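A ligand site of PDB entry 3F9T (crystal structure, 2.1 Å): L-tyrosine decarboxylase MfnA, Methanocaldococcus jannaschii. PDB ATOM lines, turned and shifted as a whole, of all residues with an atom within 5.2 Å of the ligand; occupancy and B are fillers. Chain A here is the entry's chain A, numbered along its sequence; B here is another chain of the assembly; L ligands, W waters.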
ATOM      1  N   MET A  38      15.278   7.549  -8.496  1.00  0.00           N
ATOM      2  CA  MET A  38      13.970   8.173  -8.676  1.00  0.00           C
ATOM      3  C   MET A  38      13.538   8.167 -10.131  1.00  0.00           C
ATOM      4  O   MET A  38      12.543   8.786 -10.486  1.00  0.00           O
ATOM      5  CB  MET A  38      13.935   9.572  -8.101  1.00  0.00           C
ATOM      6  CG  MET A  38      13.853   9.555  -6.575  1.00  0.00           C
ATOM      7  SD  MET A  38      13.821  11.354  -5.885  1.00  0.00           S
ATOM      8  CE  MET A  38      12.836  11.008  -4.238  1.00  0.00           C
ATOM      9  N   SER A  93      14.046  20.487 -18.320  1.00  0.00           N
ATOM     10  CA  SER A  93      15.028  19.371 -18.346  1.00  0.00           C
ATOM     11  C   SER A  93      15.017  18.456 -17.140  1.00  0.00           C
ATOM     12  O   SER A  93      15.550  17.337 -17.207  1.00  0.00           O
ATOM     13  CB  SER A  93      16.433  19.933 -18.580  1.00  0.00           C
ATOM     14  OG  SER A  93      16.823  20.767 -17.507  1.00  0.00           O
ATOM     15  N   GLY A  94      14.408  18.926 -16.060  1.00  0.00           N
ATOM     16  CA  GLY A  94      14.373  18.220 -14.809  1.00  0.00           C
ATOM     17  C   GLY A  94      14.043  19.164 -13.665  1.00  0.00           C
ATOM     18  O   GLY A  94      13.856  20.376 -13.839  1.00  0.00           O
ATOM     19  N   GLY A  95      14.000  18.573 -12.485  1.00  0.00           N
ATOM     20  CA  GLY A  95      13.734  19.281 -11.253  1.00  0.00           C
ATOM     21  C   GLY A  95      14.796  20.295 -10.904  1.00  0.00           C
ATOM     22  O   GLY A  95      14.504  21.285 -10.236  1.00  0.00           O
ATOM     23  N   THR A  96      16.028  20.081 -11.359  1.00  0.00           N
ATOM     24  CA  THR A  96      17.107  21.071 -11.111  1.00  0.00           C
ATOM     25  C   THR A  96      16.834  22.402 -11.836  1.00  0.00           C
ATOM     26  O   THR A  96      16.813  23.479 -11.222  1.00  0.00           O
ATOM     27  CB  THR A  96      18.491  20.478 -11.474  1.00  0.00           C
ATOM     28  OG1 THR A  96      18.762  19.355 -10.622  1.00  0.00           O
ATOM     29  CG2 THR A  96      19.623  21.537 -11.348  1.00  0.00           C
ATOM     30  N   GLU A  97      16.610  22.359 -13.134  1.00  0.00           N
ATOM     31  CA  GLU A  97      16.311  23.589 -13.858  1.00  0.00           C
ATOM     32  C   GLU A  97      15.055  24.246 -13.323  1.00  0.00           C
ATOM     33  O   GLU A  97      15.007  25.454 -13.199  1.00  0.00           O
ATOM     34  CB  GLU A  97      16.211  23.362 -15.360  1.00  0.00           C
ATOM     35  CG  GLU A  97      15.747  24.565 -16.131  1.00  0.00           C
ATOM     36  CD  GLU A  97      15.767  24.336 -17.647  1.00  0.00           C
ATOM     37  OE1 GLU A  97      15.725  23.142 -18.057  1.00  0.00           O
ATOM     38  OE2 GLU A  97      15.848  25.320 -18.385  1.00  0.00           O
ATOM     39  N   ASN A  99      13.746  24.126 -10.191  1.00  0.00           N
ATOM     40  CA  ASN A  99      14.151  24.786  -8.942  1.00  0.00           C
ATOM     41  C   ASN A  99      15.020  26.024  -9.196  1.00  0.00           C
ATOM     42  O   ASN A  99      14.853  27.034  -8.500  1.00  0.00           O
ATOM     43  CB  ASN A  99      14.911  23.833  -8.001  1.00  0.00           C
ATOM     44  CG  ASN A  99      14.001  22.772  -7.344  1.00  0.00           C
ATOM     45  OD1 ASN A  99      12.785  22.909  -7.294  1.00  0.00           O
ATOM     46  ND2 ASN A  99      14.632  21.736  -6.812  1.00  0.00           N
ATOM     47  N   HIS A 133      16.949  19.483  -1.755  1.00  0.00           N
ATOM     48  CA  HIS A 133      17.780  18.817  -2.761  1.00  0.00           C
ATOM     49  C   HIS A 133      19.035  19.656  -3.109  1.00  0.00           C
ATOM     50  O   HIS A 133      18.999  20.892  -3.058  1.00  0.00           O
ATOM     51  CB  HIS A 133      16.882  18.519  -3.990  1.00  0.00           C
ATOM     52  CG  HIS A 133      17.585  17.804  -5.105  1.00  0.00           C
ATOM     53  ND1 HIS A 133      18.072  18.450  -6.216  1.00  0.00           N
ATOM     54  CD2 HIS A 133      17.862  16.483  -5.290  1.00  0.00           C
ATOM     55  CE1 HIS A 133      18.661  17.574  -7.008  1.00  0.00           C
ATOM     56  NE2 HIS A 133      18.528  16.375  -6.481  1.00  0.00           N
ATOM     57  N   SER A 135      20.218  20.674  -5.814  1.00  0.00           N
ATOM     58  CA  SER A 135      19.993  21.695  -6.846  1.00  0.00           C
ATOM     59  C   SER A 135      19.929  23.068  -6.155  1.00  0.00           C
ATOM     60  O   SER A 135      20.360  24.083  -6.712  1.00  0.00           O
ATOM     61  CB  SER A 135      18.706  21.410  -7.649  1.00  0.00           C
ATOM     62  OG  SER A 135      17.578  21.127  -6.834  1.00  0.00           O
ATOM     63  N   ILE A 178       9.072  21.412   0.829  1.00  0.00           N
ATOM     64  CA  ILE A 178       9.285  20.189   0.059  1.00  0.00           C
ATOM     65  C   ILE A 178       8.123  19.210   0.214  1.00  0.00           C
ATOM     66  O   ILE A 178       7.722  18.879   1.323  1.00  0.00           O
ATOM     67  CB  ILE A 178      10.603  19.510   0.517  1.00  0.00           C
ATOM     68  CG1 ILE A 178      11.748  20.528   0.556  1.00  0.00           C
ATOM     69  CG2 ILE A 178      11.011  18.400  -0.407  1.00  0.00           C
ATOM     70  CD1 ILE A 178      12.998  19.958   1.133  1.00  0.00           C
ATOM     71  N   GLY A 180       7.656  15.732  -0.615  1.00  0.00           N
ATOM     72  CA  GLY A 180       8.285  14.449  -0.978  1.00  0.00           C
ATOM     73  C   GLY A 180       9.795  14.610  -0.991  1.00  0.00           C
ATOM     74  O   GLY A 180      10.420  14.702  -2.074  1.00  0.00           O
ATOM     75  N   THR A 181      10.393  14.657   0.205  1.00  0.00           N
ATOM     76  CA  THR A 181      11.845  14.877   0.320  1.00  0.00           C
ATOM     77  C   THR A 181      12.674  13.802  -0.412  1.00  0.00           C
ATOM     78  O   THR A 181      12.272  12.623  -0.479  1.00  0.00           O
ATOM     79  CB  THR A 181      12.360  15.065   1.790  1.00  0.00           C
ATOM     80  OG1 THR A 181      12.083  13.894   2.583  1.00  0.00           O
ATOM     81  CG2 THR A 181      11.753  16.335   2.453  1.00  0.00           C
ATOM     82  N   THR A 182      13.823  14.233  -0.929  1.00  0.00           N
ATOM     83  CA  THR A 182      14.746  13.366  -1.660  1.00  0.00           C
ATOM     84  C   THR A 182      15.159  12.145  -0.862  1.00  0.00           C
ATOM     85  O   THR A 182      15.162  11.035  -1.381  1.00  0.00           O
ATOM     86  CB  THR A 182      16.034  14.136  -2.093  1.00  0.00           C
ATOM     87  OG1 THR A 182      15.685  15.298  -2.831  1.00  0.00           O
ATOM     88  CG2 THR A 182      16.913  13.276  -2.997  1.00  0.00           C
ATOM     89  N   ASP A 207       8.947  22.292  -3.733  1.00  0.00           N
ATOM     90  CA  ASP A 207       9.638  21.309  -4.540  1.00  0.00           C
ATOM     91  C   ASP A 207       8.910  19.957  -4.435  1.00  0.00           C
ATOM     92  O   ASP A 207       9.108  19.192  -3.491  1.00  0.00           O
ATOM     93  CB  ASP A 207      11.107  21.182  -4.135  1.00  0.00           C
ATOM     94  CG  ASP A 207      11.866  20.231  -5.008  1.00  0.00           C
ATOM     95  OD1 ASP A 207      11.224  19.546  -5.862  1.00  0.00           O
ATOM     96  OD2 ASP A 207      13.119  20.183  -4.869  1.00  0.00           O
ATOM     97  N   ALA A 209       9.128  17.738  -6.995  1.00  0.00           N
ATOM     98  CA  ALA A 209       9.759  16.976  -8.090  1.00  0.00           C
ATOM     99  C   ALA A 209       9.320  15.508  -8.111  1.00  0.00           C
ATOM    100  O   ALA A 209       8.911  14.972  -9.144  1.00  0.00           O
ATOM    101  CB  ALA A 209      11.354  17.105  -8.037  1.00  0.00           C
ATOM    102  N   PHE A 210       9.367  14.869  -6.944  1.00  0.00           N
ATOM    103  CA  PHE A 210       8.983  13.471  -6.793  1.00  0.00           C
ATOM    104  C   PHE A 210       7.515  13.289  -6.331  1.00  0.00           C
ATOM    105  O   PHE A 210       6.712  12.620  -6.998  1.00  0.00           O
ATOM    106  CB  PHE A 210       9.947  12.790  -5.809  1.00  0.00           C
ATOM    107  CG  PHE A 210       9.674  11.319  -5.616  1.00  0.00           C
ATOM    108  CD1 PHE A 210      10.068  10.387  -6.572  1.00  0.00           C
ATOM    109  CD2 PHE A 210       8.990  10.875  -4.470  1.00  0.00           C
ATOM    110  CE1 PHE A 210       9.792   9.029  -6.407  1.00  0.00           C
ATOM    111  CE2 PHE A 210       8.728   9.515  -4.271  1.00  0.00           C
ATOM    112  CZ  PHE A 210       9.120   8.594  -5.248  1.00  0.00           C
ATOM    113  N   ASP A 243       8.181  16.647 -11.489  1.00  0.00           N
ATOM    114  CA  ASP A 243       8.919  15.959 -12.563  1.00  0.00           C
ATOM    115  C   ASP A 243       8.334  14.702 -13.202  1.00  0.00           C
ATOM    116  O   ASP A 243       8.407  13.620 -12.606  1.00  0.00           O
ATOM    117  CB  ASP A 243      10.292  15.547 -12.078  1.00  0.00           C
ATOM    118  CG  ASP A 243      11.227  16.731 -11.866  1.00  0.00           C
ATOM    119  OD1 ASP A 243      10.847  17.895 -12.211  1.00  0.00           O
ATOM    120  OD2 ASP A 243      12.331  16.459 -11.333  1.00  0.00           O
ATOM    121  N   HIS A 245       9.613  12.782 -15.469  1.00  0.00           N
ATOM    122  CA  HIS A 245      10.590  11.699 -15.644  1.00  0.00           C
ATOM    123  C   HIS A 245      10.951  10.954 -14.353  1.00  0.00           C
ATOM    124  O   HIS A 245      11.777  10.040 -14.364  1.00  0.00           O
ATOM    125  CB  HIS A 245      11.844  12.094 -16.449  1.00  0.00           C
ATOM    126  CG  HIS A 245      12.768  13.090 -15.808  1.00  0.00           C
ATOM    127  ND1 HIS A 245      13.448  14.033 -16.559  1.00  0.00           N
ATOM    128  CD2 HIS A 245      13.146  13.286 -14.522  1.00  0.00           C
ATOM    129  CE1 HIS A 245      14.206  14.761 -15.760  1.00  0.00           C
ATOM    130  NE2 HIS A 245      14.054  14.333 -14.520  1.00  0.00           N
ATOM    131  N   LYS A 246      10.344  11.362 -13.235  1.00  0.00           N
ATOM    132  CA  LYS A 246      10.395  10.542 -12.026  1.00  0.00           C
ATOM    133  C   LYS A 246       9.126   9.653 -12.016  1.00  0.00           C
ATOM    134  O   LYS A 246       9.061   8.694 -12.768  1.00  0.00           O
ATOM    135  CB  LYS A 246      10.558  11.409 -10.766  1.00  0.00           C
ATOM    136  CG  LYS A 246      11.929  12.138 -10.713  1.00  0.00           C
ATOM    137  CD  LYS A 246      12.010  12.990  -9.447  1.00  0.00           C
ATOM    138  CE  LYS A 246      13.354  13.632  -9.269  1.00  0.00           C
ATOM    139  NZ  LYS A 246      13.643  14.568 -10.388  1.00  0.00           N
ATOM    140  N   GLY B 285      21.190  17.735 -13.156  1.00  0.00           N
ATOM    141  CA  GLY B 285      21.420  16.506 -12.389  1.00  0.00           C
ATOM    142  C   GLY B 285      21.090  15.326 -13.283  1.00  0.00           C
ATOM    143  O   GLY B 285      21.934  14.848 -14.042  1.00  0.00           O
ATOM    144  N   THR B 286      19.849  14.846 -13.170  1.00  0.00           N
ATOM    145  CA  THR B 286      19.290  13.822 -14.061  1.00  0.00           C
ATOM    146  C   THR B 286      19.440  14.382 -15.475  1.00  0.00           C
ATOM    147  O   THR B 286      19.038  15.533 -15.734  1.00  0.00           O
ATOM    148  CB  THR B 286      17.815  13.505 -13.709  1.00  0.00           C
ATOM    149  OG1 THR B 286      17.799  12.978 -12.387  1.00  0.00           O
ATOM    150  CG2 THR B 286      17.169  12.464 -14.690  1.00  0.00           C
HETATM  151  N1  LIG L   1      14.020  18.070  -6.065  1.00  0.00           N
HETATM  152  C1  LIG L   1      13.836  16.828  -5.479  1.00  0.00           C
HETATM  153  C2  LIG L   1      12.944  16.685  -4.268  1.00  0.00           C
HETATM  154  C3  LIG L   1      14.478  15.726  -6.019  1.00  0.00           C
HETATM  155  O1  LIG L   1      14.275  14.504  -5.447  1.00  0.00           O
HETATM  156  C4  LIG L   1      15.293  15.840  -7.161  1.00  0.00           C
HETATM  157  C5  LIG L   1      15.891  14.601  -7.808  1.00  0.00           C
HETATM  158  O2  LIG L   1      16.792  13.970  -7.246  1.00  0.00           O
HETATM  159  C6  LIG L   1      15.450  17.100  -7.750  1.00  0.00           C
HETATM  160  C7  LIG L   1      14.806  18.195  -7.203  1.00  0.00           C
HETATM  161  C8  LIG L   1      16.258  17.274  -9.027  1.00  0.00           C
HETATM  162  O3  LIG L   1      15.680  16.588 -10.141  1.00  0.00           O
HETATM  163  P1  LIG L   1      16.531  16.270 -11.470  1.00  0.00           P
HETATM  164  O4  LIG L   1      17.257  17.529 -11.880  1.00  0.00           O
HETATM  165  O5  LIG L   1      15.469  15.692 -12.432  1.00  0.00           O
HETATM  166  O6  LIG L   1      17.646  15.305 -11.118  1.00  0.00           O
HETATM  167  O   HOH W   1      15.192  12.425 -11.705  1.00  0.00           O
HETATM  168  O   HOH W   2      18.514  17.757 -14.212  1.00  0.00           O
HETATM  169  O   HOH W   3       9.594  16.091  -4.279  1.00  0.00           O
HETATM  170  O   HOH W   4      19.325  13.367  -6.920  1.00  0.00           O
HETATM  171  O   HOH W   5      19.772  15.648  -9.422  1.00  0.00           O
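A nitrogen (N1) of the ligand sits close to the side-chain carboxylate (OD2) of Asp 207 (2.6 Å).
N of Thr 286 of chain B sits close to O6 of the ligand, 3.0 Å away.
The side-chain hydroxyl of Thr 286 of chain B lies close to an oxygen (O6) of the ligand, at 2.7 Å.
The backbone NH (N) of Thr 96 sits close to an oxygen (O4) of the ligand, 2.9 Å away.
The side-chain hydroxyl (OG1) of Thr 96 lies close to an oxygen (O4) of the ligand (2.7 Å).
NE2 of His 245 lies close to O5 of the ligand (2.9 Å).
The side-chain amino group (NZ) of Lys 246 sits close to an oxygen (O3) of the ligand (2.9 Å).
NE2 of His 133 sits close to O2 of the ligand (3.1 Å).
The side-chain hydroxyl (OG1) of Thr 182 sits close to an oxygen (O1) of the ligand (3.1 Å).
SD of Met 38 sits close to O1 of the ligand.
N of Gly 95 sits close to O5 of the ligand, at 3.2 Å.
OD2 of Asp 243 lies close to O5 of the ligand, 3.4 Å away.
Gly 94 touches the ligand (CA to O5, 3.6 Å).
Asn 99 touches the ligand.
O of Gly 180 touches C2 of the ligand, 3.9 Å away.
Ala 209 touches the ligand.
Hydrophobic or aromatic side chains within 4 Å of the ligand: Met 38, His 133, Ala 209 and His 245.
Within 4 Å of the ligand: Met 38, Gly 94, Gly 95, Thr 96, Asn 99, His 133, Gly 180, Thr 182, Asp 207, Ala 209, Asp 243, His 245, Lys 246 and Thr 286 of chain B.
The nearest printed residue that does not touch the ligand is Ser 135 (4.1 Å).
The backbone NH (N) of Ala 209 sits at hydrogen-bond distance from the side-chain carboxylate (OD1) of Asp 207 (3.0 Å).
OD2 of Asp 207 is in hydrogen-bond range of ND2 of Asn 99, 2.9 Å away.
NZ of Lys 246 is in salt-bridge range of OD2 of Asp 243 (2.5 Å).
A ring nitrogen (ND1) of His 133 is in hydrogen-bond range of the side-chain hydroxyl (OG) of Ser 135.
The side-chain carboxylate of Asp 243 is in hydrogen-bond range of the backbone NH of Gly 95, 2.9 Å away.
The backbone carbonyl oxygen (O) of Gly 95 lies close to the side-chain amide nitrogen (ND2) of Asn 99.
The backbone NH (N) of Asp 243 lies within hydrogen-bond range of the backbone carbonyl oxygen (O) of Ala 209 (3.0 Å).
The side-chain amide nitrogen (ND2) of Asn 99 sits at hydrogen-bond distance from the side-chain hydroxyl (OG) of Ser 135, at 3.0 Å.
Water W1 bridges the side-chain hydroxyl (OG1) of Thr 286 of chain B (2.8 Å) and the side-chain amino group (NZ) of Lys 246 (3.0 Å).
Water W3 lies within hydrogen-bond range of O of Gly 180 (2.7 Å), N of Phe 210 (2.9 Å), N of Ala 209 (3.2 Å) and O of Asp 207 (3.2 Å).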
